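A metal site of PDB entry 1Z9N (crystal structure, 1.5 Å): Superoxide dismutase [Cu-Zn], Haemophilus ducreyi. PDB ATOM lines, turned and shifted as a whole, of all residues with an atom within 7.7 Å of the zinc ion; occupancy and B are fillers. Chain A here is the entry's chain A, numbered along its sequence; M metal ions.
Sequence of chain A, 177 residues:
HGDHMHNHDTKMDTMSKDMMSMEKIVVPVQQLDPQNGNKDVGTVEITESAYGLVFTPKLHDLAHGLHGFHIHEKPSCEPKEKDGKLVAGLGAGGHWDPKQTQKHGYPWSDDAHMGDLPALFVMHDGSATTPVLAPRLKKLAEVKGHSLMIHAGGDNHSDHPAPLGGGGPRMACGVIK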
ATOM      1  N   PHE A  69      19.958 -19.115   1.009  1.00  0.00           N
ATOM      2  CA  PHE A  69      20.011 -20.161   2.020  1.00  0.00           C
ATOM      3  C   PHE A  69      18.928 -19.849   3.015  1.00  0.00           C
ATOM      4  O   PHE A  69      19.022 -18.825   3.743  1.00  0.00           O
ATOM      5  CB  PHE A  69      21.407 -20.106   2.634  1.00  0.00           C
ATOM      6  CG  PHE A  69      21.764 -21.243   3.558  1.00  0.00           C
ATOM      7  CD1 PHE A  69      21.411 -22.552   3.284  1.00  0.00           C
ATOM      8  CD2 PHE A  69      22.547 -20.997   4.674  1.00  0.00           C
ATOM      9  CE1 PHE A  69      21.801 -23.578   4.112  1.00  0.00           C
ATOM     10  CE2 PHE A  69      22.933 -22.010   5.514  1.00  0.00           C
ATOM     11  CZ  PHE A  69      22.584 -23.306   5.244  1.00  0.00           C
ATOM     12  N   HIS A  70      17.841 -20.630   2.971  1.00  0.00           N
ATOM     13  CA  HIS A  70      16.702 -20.385   3.835  1.00  0.00           C
ATOM     14  C   HIS A  70      16.096 -21.671   4.353  1.00  0.00           C
ATOM     15  O   HIS A  70      16.234 -22.729   3.725  1.00  0.00           O
ATOM     16  CB  HIS A  70      15.561 -19.608   3.114  1.00  0.00           C
ATOM     17  CG  HIS A  70      16.007 -18.745   1.989  1.00  0.00           C
ATOM     18  ND1 HIS A  70      15.839 -19.097   0.649  1.00  0.00           N
ATOM     19  CD2 HIS A  70      16.689 -17.575   1.986  1.00  0.00           C
ATOM     20  CE1 HIS A  70      16.354 -18.149  -0.113  1.00  0.00           C
ATOM     21  NE2 HIS A  70      16.887 -17.219   0.670  1.00  0.00           N
ATOM     22  N   ILE A  71      15.423 -21.552   5.504  1.00  0.00           N
ATOM     23  CA  ILE A  71      14.567 -22.605   5.993  1.00  0.00           C
ATOM     24  C   ILE A  71      13.204 -22.417   5.327  1.00  0.00           C
ATOM     25  O   ILE A  71      12.625 -21.309   5.316  1.00  0.00           O
ATOM     26  CB  ILE A  71      14.453 -22.576   7.500  1.00  0.00           C
ATOM     27  CG1 ILE A  71      15.836 -22.758   8.129  1.00  0.00           C
ATOM     28  CG2 ILE A  71      13.514 -23.700   7.974  1.00  0.00           C
ATOM     29  CD1 ILE A  71      15.822 -22.485   9.597  1.00  0.00           C
ATOM     30  N   HIS A  72      12.696 -23.506   4.745  1.00  0.00           N
ATOM     31  CA  HIS A  72      11.363 -23.497   4.139  1.00  0.00           C
ATOM     32  C   HIS A  72      10.370 -24.233   5.022  1.00  0.00           C
ATOM     33  O   HIS A  72      10.746 -24.970   5.924  1.00  0.00           O
ATOM     34  CB  HIS A  72      11.412 -24.098   2.736  1.00  0.00           C
ATOM     35  CG  HIS A  72      12.010 -23.193   1.712  1.00  0.00           C
ATOM     36  ND1 HIS A  72      11.376 -22.829   0.538  1.00  0.00           N
ATOM     37  CD2 HIS A  72      13.209 -22.549   1.700  1.00  0.00           C
ATOM     38  CE1 HIS A  72      12.173 -22.018  -0.159  1.00  0.00           C
ATOM     39  NE2 HIS A  72      13.275 -21.828   0.538  1.00  0.00           N
ATOM     40  N   GLY A  94       7.046 -22.578   0.871  1.00  0.00           N
ATOM     41  CA  GLY A  94       7.617 -21.247   0.896  1.00  0.00           C
ATOM     42  C   GLY A  94       8.627 -21.101   2.004  1.00  0.00           C
ATOM     43  O   GLY A  94       8.931 -22.037   2.743  1.00  0.00           O
ATOM     44  N   HIS A  95       9.164 -19.908   2.110  1.00  0.00           N
ATOM     45  CA  HIS A  95      10.069 -19.628   3.225  1.00  0.00           C
ATOM     46  C   HIS A  95       9.325 -19.818   4.532  1.00  0.00           C
ATOM     47  O   HIS A  95       8.125 -19.470   4.678  1.00  0.00           O
ATOM     48  CB  HIS A  95      10.601 -18.189   3.107  1.00  0.00           C
ATOM     49  CG  HIS A  95      11.536 -17.961   1.957  1.00  0.00           C
ATOM     50  ND1 HIS A  95      12.477 -16.954   1.922  1.00  0.00           N
ATOM     51  CD2 HIS A  95      11.711 -18.685   0.818  1.00  0.00           C
ATOM     52  CE1 HIS A  95      13.145 -17.029   0.780  1.00  0.00           C
ATOM     53  NE2 HIS A  95      12.683 -18.051   0.087  1.00  0.00           N
ATOM     54  N   TRP A  96      10.010 -20.399   5.513  1.00  0.00           N
ATOM     55  CA  TRP A  96       9.434 -20.590   6.838  1.00  0.00           C
ATOM     56  C   TRP A  96       9.118 -19.241   7.454  1.00  0.00           C
ATOM     57  O   TRP A  96      10.003 -18.410   7.677  1.00  0.00           O
ATOM     58  CB  TRP A  96      10.368 -21.432   7.688  1.00  0.00           C
ATOM     59  CG  TRP A  96       9.891 -21.684   9.074  1.00  0.00           C
ATOM     60  CD1 TRP A  96       8.644 -22.090   9.458  1.00  0.00           C
ATOM     61  CD2 TRP A  96      10.672 -21.585  10.246  1.00  0.00           C
ATOM     62  NE1 TRP A  96       8.618 -22.219  10.824  1.00  0.00           N
ATOM     63  CE2 TRP A  96       9.855 -21.917  11.330  1.00  0.00           C
ATOM     64  CE3 TRP A  96      12.020 -21.247  10.476  1.00  0.00           C
ATOM     65  CZ2 TRP A  96      10.308 -21.900  12.650  1.00  0.00           C
ATOM     66  CZ3 TRP A  96      12.467 -21.206  11.775  1.00  0.00           C
ATOM     67  CH2 TRP A  96      11.614 -21.573  12.851  1.00  0.00           C
ATOM     68  N   ASP A  97       7.819 -19.026   7.756  1.00  0.00           N
ATOM     69  CA  ASP A  97       7.313 -17.717   8.128  1.00  0.00           C
ATOM     70  C   ASP A  97       6.253 -17.816   9.248  1.00  0.00           C
ATOM     71  O   ASP A  97       5.079 -17.446   9.044  1.00  0.00           O
ATOM     72  CB  ASP A  97       6.760 -17.020   6.866  1.00  0.00           C
ATOM     73  CG  ASP A  97       6.438 -15.564   7.083  1.00  0.00           C
ATOM     74  OD1 ASP A  97       6.842 -14.942   8.121  1.00  0.00           O
ATOM     75  OD2 ASP A  97       5.755 -14.931   6.235  1.00  0.00           O
ATOM     76  N   THR A 101       5.227 -12.526   8.447  1.00  0.00           N
ATOM     77  CA  THR A 101       5.656 -11.212   7.974  1.00  0.00           C
ATOM     78  C   THR A 101       5.323 -11.038   6.490  1.00  0.00           C
ATOM     79  O   THR A 101       5.149  -9.929   6.021  1.00  0.00           O
ATOM     80  CB  THR A 101       7.163 -10.972   8.125  1.00  0.00           C
ATOM     81  OG1 THR A 101       7.882 -11.813   7.194  1.00  0.00           O
ATOM     82  CG2 THR A 101       7.672 -11.329   9.517  1.00  0.00           C
ATOM     83  N   LYS A 103       7.310 -11.126   4.182  1.00  0.00           N
ATOM     84  CA  LYS A 103       8.366 -10.286   3.656  1.00  0.00           C
ATOM     85  C   LYS A 103       9.693 -11.017   3.846  1.00  0.00           C
ATOM     86  O   LYS A 103      10.019 -11.441   4.973  1.00  0.00           O
ATOM     87  CB  LYS A 103       8.453  -8.926   4.392  1.00  0.00           C
ATOM     88  CG  LYS A 103       7.303  -7.997   4.114  1.00  0.00           C
ATOM     89  CD  LYS A 103       7.393  -6.670   4.880  1.00  0.00           C
ATOM     90  CE  LYS A 103       7.198  -6.821   6.404  1.00  0.00           C
ATOM     91  NZ  LYS A 103       5.904  -7.498   6.868  1.00  0.00           N
ATOM     92  N   HIS A 104      10.435 -11.116   2.768  1.00  0.00           N
ATOM     93  CA  HIS A 104      11.808 -11.653   2.804  1.00  0.00           C
ATOM     94  C   HIS A 104      12.760 -10.556   3.273  1.00  0.00           C
ATOM     95  O   HIS A 104      12.633  -9.403   2.868  1.00  0.00           O
ATOM     96  CB  HIS A 104      12.220 -12.160   1.436  1.00  0.00           C
ATOM     97  CG  HIS A 104      13.552 -12.813   1.413  1.00  0.00           C
ATOM     98  ND1 HIS A 104      13.766 -14.030   2.026  1.00  0.00           N
ATOM     99  CD2 HIS A 104      14.722 -12.401   0.904  1.00  0.00           C
ATOM    100  CE1 HIS A 104      15.057 -14.312   1.904  1.00  0.00           C
ATOM    101  NE2 HIS A 104      15.657 -13.349   1.218  1.00  0.00           N
ATOM    102  N   GLY A 105      13.697 -10.892   4.144  1.00  0.00           N
ATOM    103  CA  GLY A 105      14.588  -9.862   4.665  1.00  0.00           C
ATOM    104  C   GLY A 105      15.899 -10.366   5.232  1.00  0.00           C
ATOM    105  O   GLY A 105      16.327 -11.496   4.952  1.00  0.00           O
ATOM    106  N   TYR A 106      16.503  -9.554   6.060  1.00  0.00           N
ATOM    107  CA  TYR A 106      17.817  -9.857   6.644  1.00  0.00           C
ATOM    108  C   TYR A 106      17.663 -10.817   7.816  1.00  0.00           C
ATOM    109  O   TYR A 106      16.631 -10.826   8.486  1.00  0.00           O
ATOM    110  CB  TYR A 106      18.524  -8.574   7.031  1.00  0.00           C
ATOM    111  CG  TYR A 106      19.190  -7.892   5.846  1.00  0.00           C
ATOM    112  CD1 TYR A 106      18.684  -6.704   5.347  1.00  0.00           C
ATOM    113  CD2 TYR A 106      20.304  -8.454   5.217  1.00  0.00           C
ATOM    114  CE1 TYR A 106      19.260  -6.064   4.256  1.00  0.00           C
ATOM    115  CE2 TYR A 106      20.891  -7.826   4.108  1.00  0.00           C
ATOM    116  CZ  TYR A 106      20.369  -6.630   3.650  1.00  0.00           C
ATOM    117  OH  TYR A 106      20.928  -5.981   2.570  1.00  0.00           O
ATOM    118  N   ALA A 112      11.594  -9.947   8.846  1.00  0.00           N
ATOM    119  CA  ALA A 112      11.934 -10.960   7.850  1.00  0.00           C
ATOM    120  C   ALA A 112      11.354 -12.319   8.208  1.00  0.00           C
ATOM    121  O   ALA A 112      11.113 -12.606   9.361  1.00  0.00           O
ATOM    122  CB  ALA A 112      13.469 -11.063   7.768  1.00  0.00           C
ATOM    123  N   HIS A 113      11.160 -13.181   7.215  1.00  0.00           N
ATOM    124  CA  HIS A 113      10.793 -14.546   7.492  1.00  0.00           C
ATOM    125  C   HIS A 113      11.757 -15.174   8.520  1.00  0.00           C
ATOM    126  O   HIS A 113      12.952 -14.987   8.429  1.00  0.00           O
ATOM    127  CB  HIS A 113      10.937 -15.420   6.246  1.00  0.00           C
ATOM    128  CG  HIS A 113      10.165 -14.958   5.057  1.00  0.00           C
ATOM    129  ND1 HIS A 113      10.712 -14.921   3.788  1.00  0.00           N
ATOM    130  CD2 HIS A 113       8.863 -14.598   4.906  1.00  0.00           C
ATOM    131  CE1 HIS A 113       9.794 -14.524   2.923  1.00  0.00           C
ATOM    132  NE2 HIS A 113       8.666 -14.327   3.580  1.00  0.00           N
ATOM    133  N   MET A 114      11.240 -15.952   9.454  1.00  0.00           N
ATOM    134  CA  MET A 114      12.110 -16.591  10.427  1.00  0.00           C
ATOM    135  C   MET A 114      13.145 -17.496   9.771  1.00  0.00           C
ATOM    136  O   MET A 114      14.262 -17.705  10.280  1.00  0.00           O
ATOM    137  CB  MET A 114      11.300 -17.395  11.445  1.00  0.00           C
ATOM    138  CG  MET A 114      12.000 -17.627  12.749  1.00  0.00           C
ATOM    139  SD  MET A 114      12.276 -16.119  13.684  1.00  0.00           S
ATOM    140  CE  MET A 114      10.607 -15.659  14.077  1.00  0.00           C
ATOM    141  N   GLY A 115      12.828 -18.016   8.594  1.00  0.00           N
ATOM    142  CA  GLY A 115      13.743 -18.864   7.884  1.00  0.00           C
ATOM    143  C   GLY A 115      14.880 -18.217   7.109  1.00  0.00           C
ATOM    144  O   GLY A 115      15.642 -18.910   6.485  1.00  0.00           O
ATOM    145  N   ASP A 116      14.961 -16.894   7.111  1.00  0.00           N
ATOM    146  CA  ASP A 116      15.958 -16.169   6.334  1.00  0.00           C
ATOM    147  C   ASP A 116      17.337 -16.209   6.974  1.00  0.00           C
ATOM    148  O   ASP A 116      17.523 -15.596   8.043  1.00  0.00           O
ATOM    149  CB  ASP A 116      15.476 -14.738   6.150  1.00  0.00           C
ATOM    150  CG  ASP A 116      14.273 -14.658   5.260  1.00  0.00           C
ATOM    151  OD1 ASP A 116      13.978 -15.695   4.612  1.00  0.00           O
ATOM    152  OD2 ASP A 116      13.632 -13.598   5.112  1.00  0.00           O
ATOM    153  N   LEU A 117      18.271 -16.913   6.328  1.00  0.00           N
ATOM    154  CA  LEU A 117      19.636 -17.091   6.807  1.00  0.00           C
ATOM    155  C   LEU A 117      20.613 -16.272   5.966  1.00  0.00           C
ATOM    156  O   LEU A 117      20.257 -15.821   4.851  1.00  0.00           O
ATOM    157  CB  LEU A 117      20.021 -18.581   6.743  1.00  0.00           C
ATOM    158  CG  LEU A 117      18.988 -19.608   7.235  1.00  0.00           C
ATOM    159  CD1 LEU A 117      19.496 -21.019   7.024  1.00  0.00           C
ATOM    160  CD2 LEU A 117      18.692 -19.405   8.667  1.00  0.00           C
ATOM    161  N   ARG A 136      18.253 -14.908  15.280  1.00  0.00           N
ATOM    162  CA  ARG A 136      16.895 -14.944  15.810  1.00  0.00           C
ATOM    163  C   ARG A 136      16.479 -16.304  16.297  1.00  0.00           C
ATOM    164  O   ARG A 136      15.473 -16.430  17.023  1.00  0.00           O
ATOM    165  CB  ARG A 136      15.903 -14.449  14.766  1.00  0.00           C
ATOM    166  CG  ARG A 136      16.038 -12.993  14.507  1.00  0.00           C
ATOM    167  CD  ARG A 136      14.960 -12.447  13.605  1.00  0.00           C
ATOM    168  NE  ARG A 136      15.237 -12.838  12.254  1.00  0.00           N
ATOM    169  CZ  ARG A 136      14.333 -13.141  11.315  1.00  0.00           C
ATOM    170  NH1 ARG A 136      13.018 -13.133  11.556  1.00  0.00           N
ATOM    171  NH2 ARG A 136      14.780 -13.452  10.100  1.00  0.00           N
ATOM    172  N   ASP A 155      21.168 -13.858  -2.666  1.00  0.00           N
ATOM    173  CA  ASP A 155      20.199 -13.329  -1.739  1.00  0.00           C
ATOM    174  C   ASP A 155      20.573 -11.908  -1.369  1.00  0.00           C
ATOM    175  O   ASP A 155      21.512 -11.686  -0.625  1.00  0.00           O
ATOM    176  CB  ASP A 155      20.123 -14.194  -0.471  1.00  0.00           C
ATOM    177  CG  ASP A 155      18.837 -14.001   0.324  1.00  0.00           C
ATOM    178  OD1 ASP A 155      18.130 -12.968   0.149  1.00  0.00           O
ATOM    179  OD2 ASP A 155      18.503 -14.834   1.190  1.00  0.00           O
ATOM    180  N   HIS A 157      18.426 -10.169   0.355  1.00  0.00           N
ATOM    181  CA  HIS A 157      17.631 -10.006   1.552  1.00  0.00           C
ATOM    182  C   HIS A 157      16.491  -8.976   1.386  1.00  0.00           C
ATOM    183  O   HIS A 157      16.166  -8.252   2.309  1.00  0.00           O
ATOM    184  CB  HIS A 157      18.490  -9.688   2.764  1.00  0.00           C
ATOM    185  CG  HIS A 157      19.427 -10.798   3.078  1.00  0.00           C
ATOM    186  ND1 HIS A 157      19.009 -11.998   3.593  1.00  0.00           N
ATOM    187  CD2 HIS A 157      20.727 -10.966   2.748  1.00  0.00           C
ATOM    188  CE1 HIS A 157      20.064 -12.810   3.700  1.00  0.00           C
ATOM    189  NE2 HIS A 157      21.105 -12.199   3.186  1.00  0.00           N
ATOM    190  N   SER A 158      15.961  -8.950   0.173  1.00  0.00           N
ATOM    191  CA  SER A 158      14.789  -8.148  -0.144  1.00  0.00           C
ATOM    192  C   SER A 158      13.918  -8.908  -1.122  1.00  0.00           C
ATOM    193  O   SER A 158      14.357  -9.839  -1.796  1.00  0.00           O
ATOM    194  CB  SER A 158      15.246  -6.836  -0.791  1.00  0.00           C
ATOM    195  OG  SER A 158      14.140  -6.041  -1.198  1.00  0.00           O
ATOM    196  N   ASP A 159      12.672  -8.458  -1.243  1.00  0.00           N
ATOM    197  CA  ASP A 159      11.813  -8.977  -2.295  1.00  0.00           C
ATOM    198  C   ASP A 159      11.878  -8.181  -3.603  1.00  0.00           C
ATOM    199  O   ASP A 159      11.108  -8.436  -4.547  1.00  0.00           O
ATOM    200  CB  ASP A 159      10.363  -9.000  -1.774  1.00  0.00           C
ATOM    201  CG  ASP A 159      10.104 -10.141  -0.817  1.00  0.00           C
ATOM    202  OD1 ASP A 159      10.424 -11.311  -1.196  1.00  0.00           O
ATOM    203  OD2 ASP A 159       9.560  -9.960   0.310  1.00  0.00           O
ATOM    204  N   LEU A 164      11.987 -12.860  -2.953  1.00  0.00           N
ATOM    205  CA  LEU A 164      12.674 -13.845  -2.131  1.00  0.00           C
ATOM    206  C   LEU A 164      14.182 -13.754  -2.299  1.00  0.00           C
ATOM    207  O   LEU A 164      14.891 -14.775  -2.267  1.00  0.00           O
ATOM    208  CB  LEU A 164      12.133 -15.241  -2.401  1.00  0.00           C
ATOM    209  CG  LEU A 164      10.630 -15.341  -2.053  1.00  0.00           C
ATOM    210  CD1 LEU A 164      10.143 -16.704  -2.484  1.00  0.00           C
ATOM    211  CD2 LEU A 164      10.301 -15.075  -0.597  1.00  0.00           C
ATOM    212  N   GLY A 165      14.672 -12.536  -2.461  1.00  0.00           N
ATOM    213  CA  GLY A 165      16.129 -12.335  -2.538  1.00  0.00           C
ATOM    214  C   GLY A 165      16.798 -12.580  -3.853  1.00  0.00           C
ATOM    215  O   GLY A 165      18.017 -12.424  -3.962  1.00  0.00           O
HETATM  216 ZN    ZN M   1      12.636 -15.333   3.170  1.00  0.00          ZN
HETATM  217 CU    CU M   2      14.692 -20.577  -0.043  1.00  0.00          CU
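A ring nitrogen (NE2) of His 104 is in hydrogen-bond range of the side-chain carboxylate (OD1) of Asp 155, at 2.7 Å. OD2 of Asp 116 lies within hydrogen-bond range of N of Gly 105 (2.9 Å). OD2 of Asp 159 lies within hydrogen-bond range of N of His 104 (2.9 Å). The backbone NH (N) of His 113 sits at hydrogen-bond distance from the backbone carbonyl oxygen (O) of Lys 103 (3.1 Å). The backbone carbonyl oxygen of His 113 is in hydrogen-bond range of the guanidinium group of Arg 136, at 2.9 Å. ND1 of His 70 sits close to NE2 of His 95 (3.4 Å).
Within 4 Å of the zinc ion: His 95, His 104, His 113 and Asp 116.
The zinc ion is bound by the side-chain carboxylate (OD1) of Asp 116. A ring nitrogen (ND1) of His 95 is bound to the zinc ion, at 2.1 Å. ND1 of His 113 is bound to the zinc ion, 2.1 Å away. A ring nitrogen (ND1) of His 104 is bound to the zinc ion. The zinc ion has four donor atoms within binding distance. Slightly farther from the zinc ion lies OD2 of Asp 116 (2.8 Å).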
